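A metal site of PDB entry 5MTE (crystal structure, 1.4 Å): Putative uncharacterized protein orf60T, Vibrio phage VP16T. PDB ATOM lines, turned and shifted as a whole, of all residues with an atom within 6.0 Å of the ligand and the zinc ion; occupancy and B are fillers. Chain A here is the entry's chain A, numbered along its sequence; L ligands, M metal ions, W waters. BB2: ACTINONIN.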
ATOM      1  N   ALA A  38       4.163  -6.899  14.069  1.00  0.00           N
ATOM      2  CA  ALA A  38       5.544  -7.252  14.436  1.00  0.00           C
ATOM      3  C   ALA A  38       6.588  -6.768  13.422  1.00  0.00           C
ATOM      4  O   ALA A  38       7.793  -6.949  13.625  1.00  0.00           O
ATOM      5  CB  ALA A  38       5.666  -8.744  14.642  1.00  0.00           C
ATOM      6  N   GLY A  39       6.128  -6.165  12.327  1.00  0.00           N
ATOM      7  CA  GLY A  39       7.023  -5.606  11.314  1.00  0.00           C
ATOM      8  C   GLY A  39       7.644  -6.627  10.391  1.00  0.00           C
ATOM      9  O   GLY A  39       8.766  -6.435   9.900  1.00  0.00           O
ATOM     10  N   GLY A  40       6.934  -7.713  10.127  1.00  0.00           N
ATOM     11  CA  GLY A  40       7.466  -8.763   9.266  1.00  0.00           C
ATOM     12  C   GLY A  40       6.957  -8.686   7.837  1.00  0.00           C
ATOM     13  O   GLY A  40       6.001  -7.949   7.562  1.00  0.00           O
ATOM     14  N   ILE A  41       7.632  -9.401   6.937  1.00  0.00           N
ATOM     15  CA  ILE A  41       7.166  -9.514   5.535  1.00  0.00           C
ATOM     16  C   ILE A  41       6.593 -10.899   5.224  1.00  0.00           C
ATOM     17  O   ILE A  41       6.155 -11.168   4.114  1.00  0.00           O
ATOM     18  CB  ILE A  41       8.254  -9.115   4.504  1.00  0.00           C
ATOM     19  CG1 ILE A  41       9.481 -10.018   4.615  1.00  0.00           C
ATOM     20  CG2 ILE A  41       8.621  -7.644   4.668  1.00  0.00           C
ATOM     21  CD1 ILE A  41      10.521  -9.790   3.525  1.00  0.00           C
ATOM     22  N   GLY A  42       6.565 -11.763   6.237  1.00  0.00           N
ATOM     23  CA  GLY A  42       5.926 -13.074   6.144  1.00  0.00           C
ATOM     24  C   GLY A  42       5.637 -13.585   7.534  1.00  0.00           C
ATOM     25  O   GLY A  42       6.172 -13.079   8.505  1.00  0.00           O
ATOM     26  N   LEU A  43       4.756 -14.592   7.607  1.00  0.00           N
ATOM     27  CA  LEU A  43       4.463 -15.263   8.867  1.00  0.00           C
ATOM     28  C   LEU A  43       3.875 -16.623   8.561  1.00  0.00           C
ATOM     29  O   LEU A  43       3.193 -16.793   7.552  1.00  0.00           O
ATOM     30  CB  LEU A  43       3.504 -14.422   9.722  1.00  0.00           C
ATOM     31  CG  LEU A  43       3.432 -14.770  11.212  1.00  0.00           C
ATOM     32  CD1 LEU A  43       4.689 -14.245  11.909  1.00  0.00           C
ATOM     33  CD2 LEU A  43       2.202 -14.145  11.863  1.00  0.00           C
ATOM     34  N   ALA A  44       4.143 -17.578   9.445  1.00  0.00           N
ATOM     35  CA  ALA A  44       3.639 -18.938   9.315  1.00  0.00           C
ATOM     36  C   ALA A  44       2.823 -19.299  10.547  1.00  0.00           C
ATOM     37  O   ALA A  44       3.088 -18.792  11.648  1.00  0.00           O
ATOM     38  CB  ALA A  44       4.811 -19.910   9.188  1.00  0.00           C
ATOM     39  N   GLN A  47       4.229 -19.792  14.133  1.00  0.00           N
ATOM     40  CA  GLN A  47       4.766 -18.642  14.886  1.00  0.00           C
ATOM     41  C   GLN A  47       3.765 -17.990  15.810  1.00  0.00           C
ATOM     42  O   GLN A  47       4.151 -17.262  16.737  1.00  0.00           O
ATOM     43  CB  GLN A  47       5.317 -17.589  13.946  1.00  0.00           C
ATOM     44  CG  GLN A  47       6.522 -18.046  13.169  1.00  0.00           C
ATOM     45  CD  GLN A  47       6.965 -16.972  12.211  1.00  0.00           C
ATOM     46  OE1 GLN A  47       6.391 -16.806  11.134  1.00  0.00           O
ATOM     47  NE2 GLN A  47       7.985 -16.210  12.604  1.00  0.00           N
ATOM     48  N   SER A  81      21.157 -15.543   1.325  1.00  0.00           N
ATOM     49  CA  SER A  81      19.991 -14.804   1.782  1.00  0.00           C
ATOM     50  C   SER A  81      20.126 -14.430   3.267  1.00  0.00           C
ATOM     51  O   SER A  81      19.939 -15.283   4.117  1.00  0.00           O
ATOM     52  CB  SER A  81      18.738 -15.662   1.593  1.00  0.00           C
ATOM     53  OG  SER A  81      17.588 -15.068   2.192  1.00  0.00           O
ATOM     54  N   PRO A  82      20.429 -13.154   3.577  1.00  0.00           N
ATOM     55  CA  PRO A  82      20.518 -12.775   4.999  1.00  0.00           C
ATOM     56  C   PRO A  82      19.112 -12.618   5.581  1.00  0.00           C
ATOM     57  O   PRO A  82      18.309 -11.853   5.045  1.00  0.00           O
ATOM     58  CB  PRO A  82      21.291 -11.456   4.960  1.00  0.00           C
ATOM     59  CG  PRO A  82      20.974 -10.865   3.592  1.00  0.00           C
ATOM     60  CD  PRO A  82      20.717 -12.016   2.671  1.00  0.00           C
ATOM     61  N   GLU A  83      18.828 -13.337   6.669  1.00  0.00           N
ATOM     62  CA  GLU A  83      17.466 -13.377   7.187  1.00  0.00           C
ATOM     63  C   GLU A  83      17.420 -13.201   8.685  1.00  0.00           C
ATOM     64  O   GLU A  83      18.242 -13.780   9.406  1.00  0.00           O
ATOM     65  CB  GLU A  83      16.820 -14.718   6.835  1.00  0.00           C
ATOM     66  CG  GLU A  83      16.802 -15.000   5.335  1.00  0.00           C
ATOM     67  CD  GLU A  83      16.139 -16.304   4.968  1.00  0.00           C
ATOM     68  OE1 GLU A  83      15.464 -16.902   5.841  1.00  0.00           O
ATOM     69  OE2 GLU A  83      16.285 -16.730   3.792  1.00  0.00           O
ATOM     70  N   GLY A  84      16.466 -12.399   9.141  1.00  0.00           N
ATOM     71  CA  GLY A  84      16.059 -12.416  10.525  1.00  0.00           C
ATOM     72  C   GLY A  84      14.693 -13.073  10.589  1.00  0.00           C
ATOM     73  O   GLY A  84      14.026 -13.288   9.554  1.00  0.00           O
ATOM     74  N   CYS A  85      14.261 -13.389  11.802  1.00  0.00           N
ATOM     75  CA  CYS A  85      12.999 -14.062  12.026  1.00  0.00           C
ATOM     76  C   CYS A  85      12.287 -13.398  13.177  1.00  0.00           C
ATOM     77  O   CYS A  85      12.918 -13.109  14.190  1.00  0.00           O
ATOM     78  CB  CYS A  85      13.239 -15.550  12.324  1.00  0.00           C
ATOM     79  SG  CYS A  85      11.699 -16.519  12.571  1.00  0.00           S
ATOM     80  N   LEU A  86      10.984 -13.170  13.029  1.00  0.00           N
ATOM     81  CA  LEU A  86      10.212 -12.527  14.093  1.00  0.00           C
ATOM     82  C   LEU A  86      10.170 -13.355  15.369  1.00  0.00           C
ATOM     83  O   LEU A  86       9.939 -12.807  16.437  1.00  0.00           O
ATOM     84  CB  LEU A  86       8.774 -12.268  13.633  1.00  0.00           C
ATOM     85  CG  LEU A  86       8.574 -11.241  12.526  1.00  0.00           C
ATOM     86  CD1 LEU A  86       7.083 -11.200  12.184  1.00  0.00           C
ATOM     87  CD2 LEU A  86       9.102  -9.900  12.961  1.00  0.00           C
ATOM     88  N   SER A  87      10.390 -14.655  15.253  1.00  0.00           N
ATOM     89  CA  SER A  87      10.391 -15.533  16.428  1.00  0.00           C
ATOM     90  C   SER A  87      11.718 -15.479  17.180  1.00  0.00           C
ATOM     91  O   SER A  87      11.745 -15.895  18.336  1.00  0.00           O
ATOM     92  CB  SER A  87      10.091 -16.962  16.012  1.00  0.00           C
ATOM     93  OG  SER A  87       8.828 -17.019  15.379  1.00  0.00           O
ATOM     94  N   LYS A  91      18.632 -11.697  15.824  1.00  0.00           N
ATOM     95  CA  LYS A  91      19.519 -12.638  15.129  1.00  0.00           C
ATOM     96  C   LYS A  91      19.367 -12.411  13.619  1.00  0.00           C
ATOM     97  O   LYS A  91      18.253 -12.382  13.134  1.00  0.00           O
ATOM     98  CB  LYS A  91      19.069 -14.093  15.470  1.00  0.00           C
ATOM     99  CG  LYS A  91      19.896 -15.240  14.891  1.00  0.00           C
ATOM    100  CD  LYS A  91      19.092 -16.564  14.757  1.00  0.00           C
ATOM    101  CE  LYS A  91      19.138 -17.406  16.005  1.00  0.00           C
ATOM    102  NZ  LYS A  91      19.044 -18.832  15.587  1.00  0.00           N
ATOM    103  N   THR A  92      20.487 -12.273  12.904  1.00  0.00           N
ATOM    104  CA  THR A  92      20.452 -12.374  11.434  1.00  0.00           C
ATOM    105  C   THR A  92      21.376 -13.502  11.002  1.00  0.00           C
ATOM    106  O   THR A  92      22.520 -13.582  11.476  1.00  0.00           O
ATOM    107  CB  THR A  92      20.876 -11.054  10.751  1.00  0.00           C
ATOM    108  OG1 THR A  92      20.080  -9.988  11.279  1.00  0.00           O
ATOM    109  CG2 THR A  92      20.701 -11.154   9.236  1.00  0.00           C
ATOM    110  N   LEU A 120      14.219 -12.106  -3.113  1.00  0.00           N
ATOM    111  CA  LEU A 120      13.627 -11.931  -1.792  1.00  0.00           C
ATOM    112  C   LEU A 120      12.294 -12.665  -1.614  1.00  0.00           C
ATOM    113  O   LEU A 120      12.089 -13.331  -0.601  1.00  0.00           O
ATOM    114  CB  LEU A 120      13.477 -10.452  -1.448  1.00  0.00           C
ATOM    115  CG  LEU A 120      12.901 -10.160  -0.055  1.00  0.00           C
ATOM    116  CD1 LEU A 120      13.694 -10.808   1.073  1.00  0.00           C
ATOM    117  CD2 LEU A 120      12.796  -8.647   0.155  1.00  0.00           C
ATOM    118  N   PHE A 123      12.902 -16.222  -1.236  1.00  0.00           N
ATOM    119  CA  PHE A 123      13.499 -16.466   0.077  1.00  0.00           C
ATOM    120  C   PHE A 123      12.409 -16.481   1.146  1.00  0.00           C
ATOM    121  O   PHE A 123      12.406 -17.347   2.021  1.00  0.00           O
ATOM    122  CB  PHE A 123      14.538 -15.386   0.432  1.00  0.00           C
ATOM    123  CG  PHE A 123      15.648 -15.222  -0.586  1.00  0.00           C
ATOM    124  CD1 PHE A 123      16.373 -14.035  -0.632  1.00  0.00           C
ATOM    125  CD2 PHE A 123      15.976 -16.254  -1.468  1.00  0.00           C
ATOM    126  CE1 PHE A 123      17.404 -13.873  -1.556  1.00  0.00           C
ATOM    127  CE2 PHE A 123      17.003 -16.090  -2.414  1.00  0.00           C
ATOM    128  CZ  PHE A 123      17.719 -14.889  -2.453  1.00  0.00           C
ATOM    129  N   CYS A 124      11.494 -15.504   1.080  1.00  0.00           N
ATOM    130  CA  CYS A 124      10.396 -15.450   2.052  1.00  0.00           C
ATOM    131  C   CYS A 124       9.555 -16.726   2.031  1.00  0.00           C
ATOM    132  O   CYS A 124       9.240 -17.300   3.076  1.00  0.00           O
ATOM    133  CB  CYS A 124       9.424 -14.303   1.780  1.00  0.00           C
ATOM    134  SG  CYS A 124       9.987 -12.602   1.541  1.00  0.00           S
ATOM    135  N   LEU A 125       9.139 -17.144   0.828  1.00  0.00           N
ATOM    136  CA  LEU A 125       8.360 -18.372   0.707  1.00  0.00           C
ATOM    137  C   LEU A 125       9.066 -19.559   1.337  1.00  0.00           C
ATOM    138  O   LEU A 125       8.456 -20.347   2.068  1.00  0.00           O
ATOM    139  CB  LEU A 125       8.031 -18.658  -0.757  1.00  0.00           C
ATOM    140  CG  LEU A 125       6.981 -17.706  -1.330  1.00  0.00           C
ATOM    141  CD1 LEU A 125       7.011 -17.677  -2.861  1.00  0.00           C
ATOM    142  CD2 LEU A 125       5.576 -18.055  -0.844  1.00  0.00           C
ATOM    143  N   HIS A 127      11.390 -19.480   3.667  1.00  0.00           N
ATOM    144  CA  HIS A 127      11.469 -19.213   5.121  1.00  0.00           C
ATOM    145  C   HIS A 127      10.166 -19.631   5.801  1.00  0.00           C
ATOM    146  O   HIS A 127      10.186 -20.312   6.840  1.00  0.00           O
ATOM    147  CB  HIS A 127      11.766 -17.724   5.329  1.00  0.00           C
ATOM    148  CG  HIS A 127      11.888 -17.292   6.768  1.00  0.00           C
ATOM    149  ND1 HIS A 127      13.076 -16.867   7.327  1.00  0.00           N
ATOM    150  CD2 HIS A 127      10.954 -17.161   7.737  1.00  0.00           C
ATOM    151  CE1 HIS A 127      12.874 -16.522   8.585  1.00  0.00           C
ATOM    152  NE2 HIS A 127      11.590 -16.691   8.858  1.00  0.00           N
ATOM    153  N   GLU A 128       9.027 -19.246   5.204  1.00  0.00           N
ATOM    154  CA  GLU A 128       7.723 -19.536   5.828  1.00  0.00           C
ATOM    155  C   GLU A 128       7.364 -21.023   5.738  1.00  0.00           C
ATOM    156  O   GLU A 128       6.823 -21.600   6.696  1.00  0.00           O
ATOM    157  CB  GLU A 128       6.596 -18.695   5.218  1.00  0.00           C
ATOM    158  CG  GLU A 128       6.787 -17.168   5.254  1.00  0.00           C
ATOM    159  CD  GLU A 128       7.293 -16.616   6.598  1.00  0.00           C
ATOM    160  OE1 GLU A 128       7.081 -17.261   7.661  1.00  0.00           O
ATOM    161  OE2 GLU A 128       7.881 -15.514   6.562  1.00  0.00           O
ATOM    162  N   HIS A 131       9.106 -22.901   8.373  1.00  0.00           N
ATOM    163  CA  HIS A 131       8.439 -22.818   9.668  1.00  0.00           C
ATOM    164  C   HIS A 131       7.390 -23.915   9.826  1.00  0.00           C
ATOM    165  O   HIS A 131       7.250 -24.478  10.914  1.00  0.00           O
ATOM    166  CB  HIS A 131       7.722 -21.481   9.876  1.00  0.00           C
ATOM    167  CG  HIS A 131       8.579 -20.376  10.422  1.00  0.00           C
ATOM    168  ND1 HIS A 131       9.132 -20.417  11.685  1.00  0.00           N
ATOM    169  CD2 HIS A 131       8.946 -19.191   9.885  1.00  0.00           C
ATOM    170  CE1 HIS A 131       9.802 -19.297  11.896  1.00  0.00           C
ATOM    171  NE2 HIS A 131       9.696 -18.537  10.822  1.00  0.00           N
ATOM    172  N   ILE A 137      15.645 -20.516  11.313  1.00  0.00           N
ATOM    173  CA  ILE A 137      16.975 -20.013  10.915  1.00  0.00           C
ATOM    174  C   ILE A 137      18.049 -20.241  11.985  1.00  0.00           C
ATOM    175  O   ILE A 137      17.756 -20.222  13.180  1.00  0.00           O
ATOM    176  CB  ILE A 137      16.926 -18.523  10.470  1.00  0.00           C
ATOM    177  CG1 ILE A 137      16.553 -17.604  11.644  1.00  0.00           C
ATOM    178  CG2 ILE A 137      15.965 -18.323   9.264  1.00  0.00           C
ATOM    179  CD1 ILE A 137      16.739 -16.104  11.339  1.00  0.00           C
ATOM    180  OXT ILE A 137      19.240 -20.385  11.586  1.00  0.00           O
HETATM  181  C5  BB2 L   1       9.423 -12.707   9.221  1.00  0.00           C
HETATM  182  C3  BB2 L   1       9.395 -14.116   9.768  1.00  0.00           C
HETATM  183  O4  BB2 L   1       9.997 -14.455  10.786  1.00  0.00           O
HETATM  184  N1  BB2 L   1       8.689 -14.978   9.045  1.00  0.00           N
HETATM  185  O2  BB2 L   1       8.644 -16.253   9.480  1.00  0.00           O
HETATM  186  C6  BB2 L   1      10.729 -12.506   8.446  1.00  0.00           C
HETATM  187  C12 BB2 L   1      11.077 -11.037   8.266  1.00  0.00           C
HETATM  188  O13 BB2 L   1      10.224 -10.184   7.982  1.00  0.00           O
HETATM  189  C7  BB2 L   1      10.614 -13.138   7.037  1.00  0.00           C
HETATM  190  C8  BB2 L   1      11.976 -13.185   6.337  1.00  0.00           C
HETATM  191  C9  BB2 L   1      11.900 -13.894   4.982  1.00  0.00           C
HETATM  192  C10 BB2 L   1      13.270 -13.985   4.285  1.00  0.00           C
HETATM  193  C11 BB2 L   1      14.005 -12.647   4.329  1.00  0.00           C
HETATM  194  N14 BB2 L   1      12.377 -10.806   8.417  1.00  0.00           N
HETATM  195  C15 BB2 L   1      12.998  -9.499   8.206  1.00  0.00           C
HETATM  196  C16 BB2 L   1      13.456  -8.785   9.502  1.00  0.00           C
HETATM  197  C18 BB2 L   1      12.308  -8.593  10.498  1.00  0.00           C
HETATM  198  C17 BB2 L   1      14.604  -9.489  10.195  1.00  0.00           C
HETATM  199  C19 BB2 L   1      14.154  -9.767   7.215  1.00  0.00           C
HETATM  200  O20 BB2 L   1      14.911 -10.743   7.355  1.00  0.00           O
HETATM  201  N21 BB2 L   1      14.344  -8.989   6.142  1.00  0.00           N
HETATM  202  C22 BB2 L   1      15.424  -9.215   5.161  1.00  0.00           C
HETATM  203  C23 BB2 L   1      13.515  -7.818   5.802  1.00  0.00           C
HETATM  204  C24 BB2 L   1      14.220  -7.186   4.605  1.00  0.00           C
HETATM  205  C25 BB2 L   1      15.003  -8.349   3.974  1.00  0.00           C
HETATM  206  C26 BB2 L   1      16.767  -8.752   5.748  1.00  0.00           C
HETATM  207  O27 BB2 L   1      17.839  -9.221   4.929  1.00  0.00           O
HETATM  208 ZN    ZN M   1      10.473 -16.567  10.607  1.00  0.00          ZN
HETATM  209  O   HOH W   1      17.600  -9.169  10.632  1.00  0.00           O
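The zinc ion is bound by a ring nitrogen (NE2) of His 127 (2.1 Å), a ring nitrogen (NE2) of His 131 (2.1 Å), an oxygen (O2) of the ligand (2.2 Å), an oxygen (O4) of the ligand (2.2 Å) and the side-chain sulfur of Cys 85 (2.3 Å). The zinc ion has five donor atoms within binding distance.
CA of Gly 40 touches O13 of the ligand, 3.4 Å away. CA of Glu 83 touches O20 of the ligand, 3.7 Å away. Leu 120 touches the ligand. CA of Cys 124 touches C9 of the ligand (3.6 Å). Hydrophobic or aromatic side chains that line the ligand: Ile 41, Pro 82, Leu 86, Leu 120, His 127 and His 131. Of the 25 residues printed, 14 come within 4 Å of the ligand.
A ring nitrogen (ND1) of His 127 lies within hydrogen-bond range of the side-chain carboxylate (OE1) of Glu 83 (2.8 Å). SG of Cys 85 sits close to N of Ser 87, at 3.5 Å. The backbone NH of Ala 44 is in hydrogen-bond range of the side-chain carboxylate of Glu 128 (3.5 Å). OE2 of Glu 128 sits close to N of Leu 43. OE1 of Gln 47 lies within hydrogen-bond range of N of Ala 44, 2.9 Å away. The side-chain carboxylate of Glu 83 sits at hydrogen-bond distance from the side-chain hydroxyl of Ser 81 (2.6 Å). The side-chain amide nitrogen (NE2) of Gln 47 lies close to the side-chain sulfur (SG) of Cys 85. OG of Ser 87 sits at hydrogen-bond distance from NE2 of Gln 47, 3.0 Å away.
Gln 47 touches the zinc ion (NE2 to ZN, 3.2 Å).
O of Pro 82 lies within hydrogen-bond range of O27 of the ligand (2.7 Å). The backbone carbonyl oxygen (O) of Gly 42 is in hydrogen-bond range of a nitrogen (N1) of the ligand (3.2 Å). N14 of the ligand lies within hydrogen-bond range of O of Gly 84 (3.2 Å). O20 of the ligand sits at hydrogen-bond distance from N of Gly 84, 2.9 Å away. O13 of the ligand sits at hydrogen-bond distance from N of Ile 41. OE2 of Glu 128 lies within hydrogen-bond range of N1 of the ligand. The backbone NH (N) of Leu 86 lies close to an oxygen (O4) of the ligand (2.8 Å). The side-chain amide oxygen (OE1) of Gln 47 sits close to an oxygen (O2) of the ligand, 2.8 Å away.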
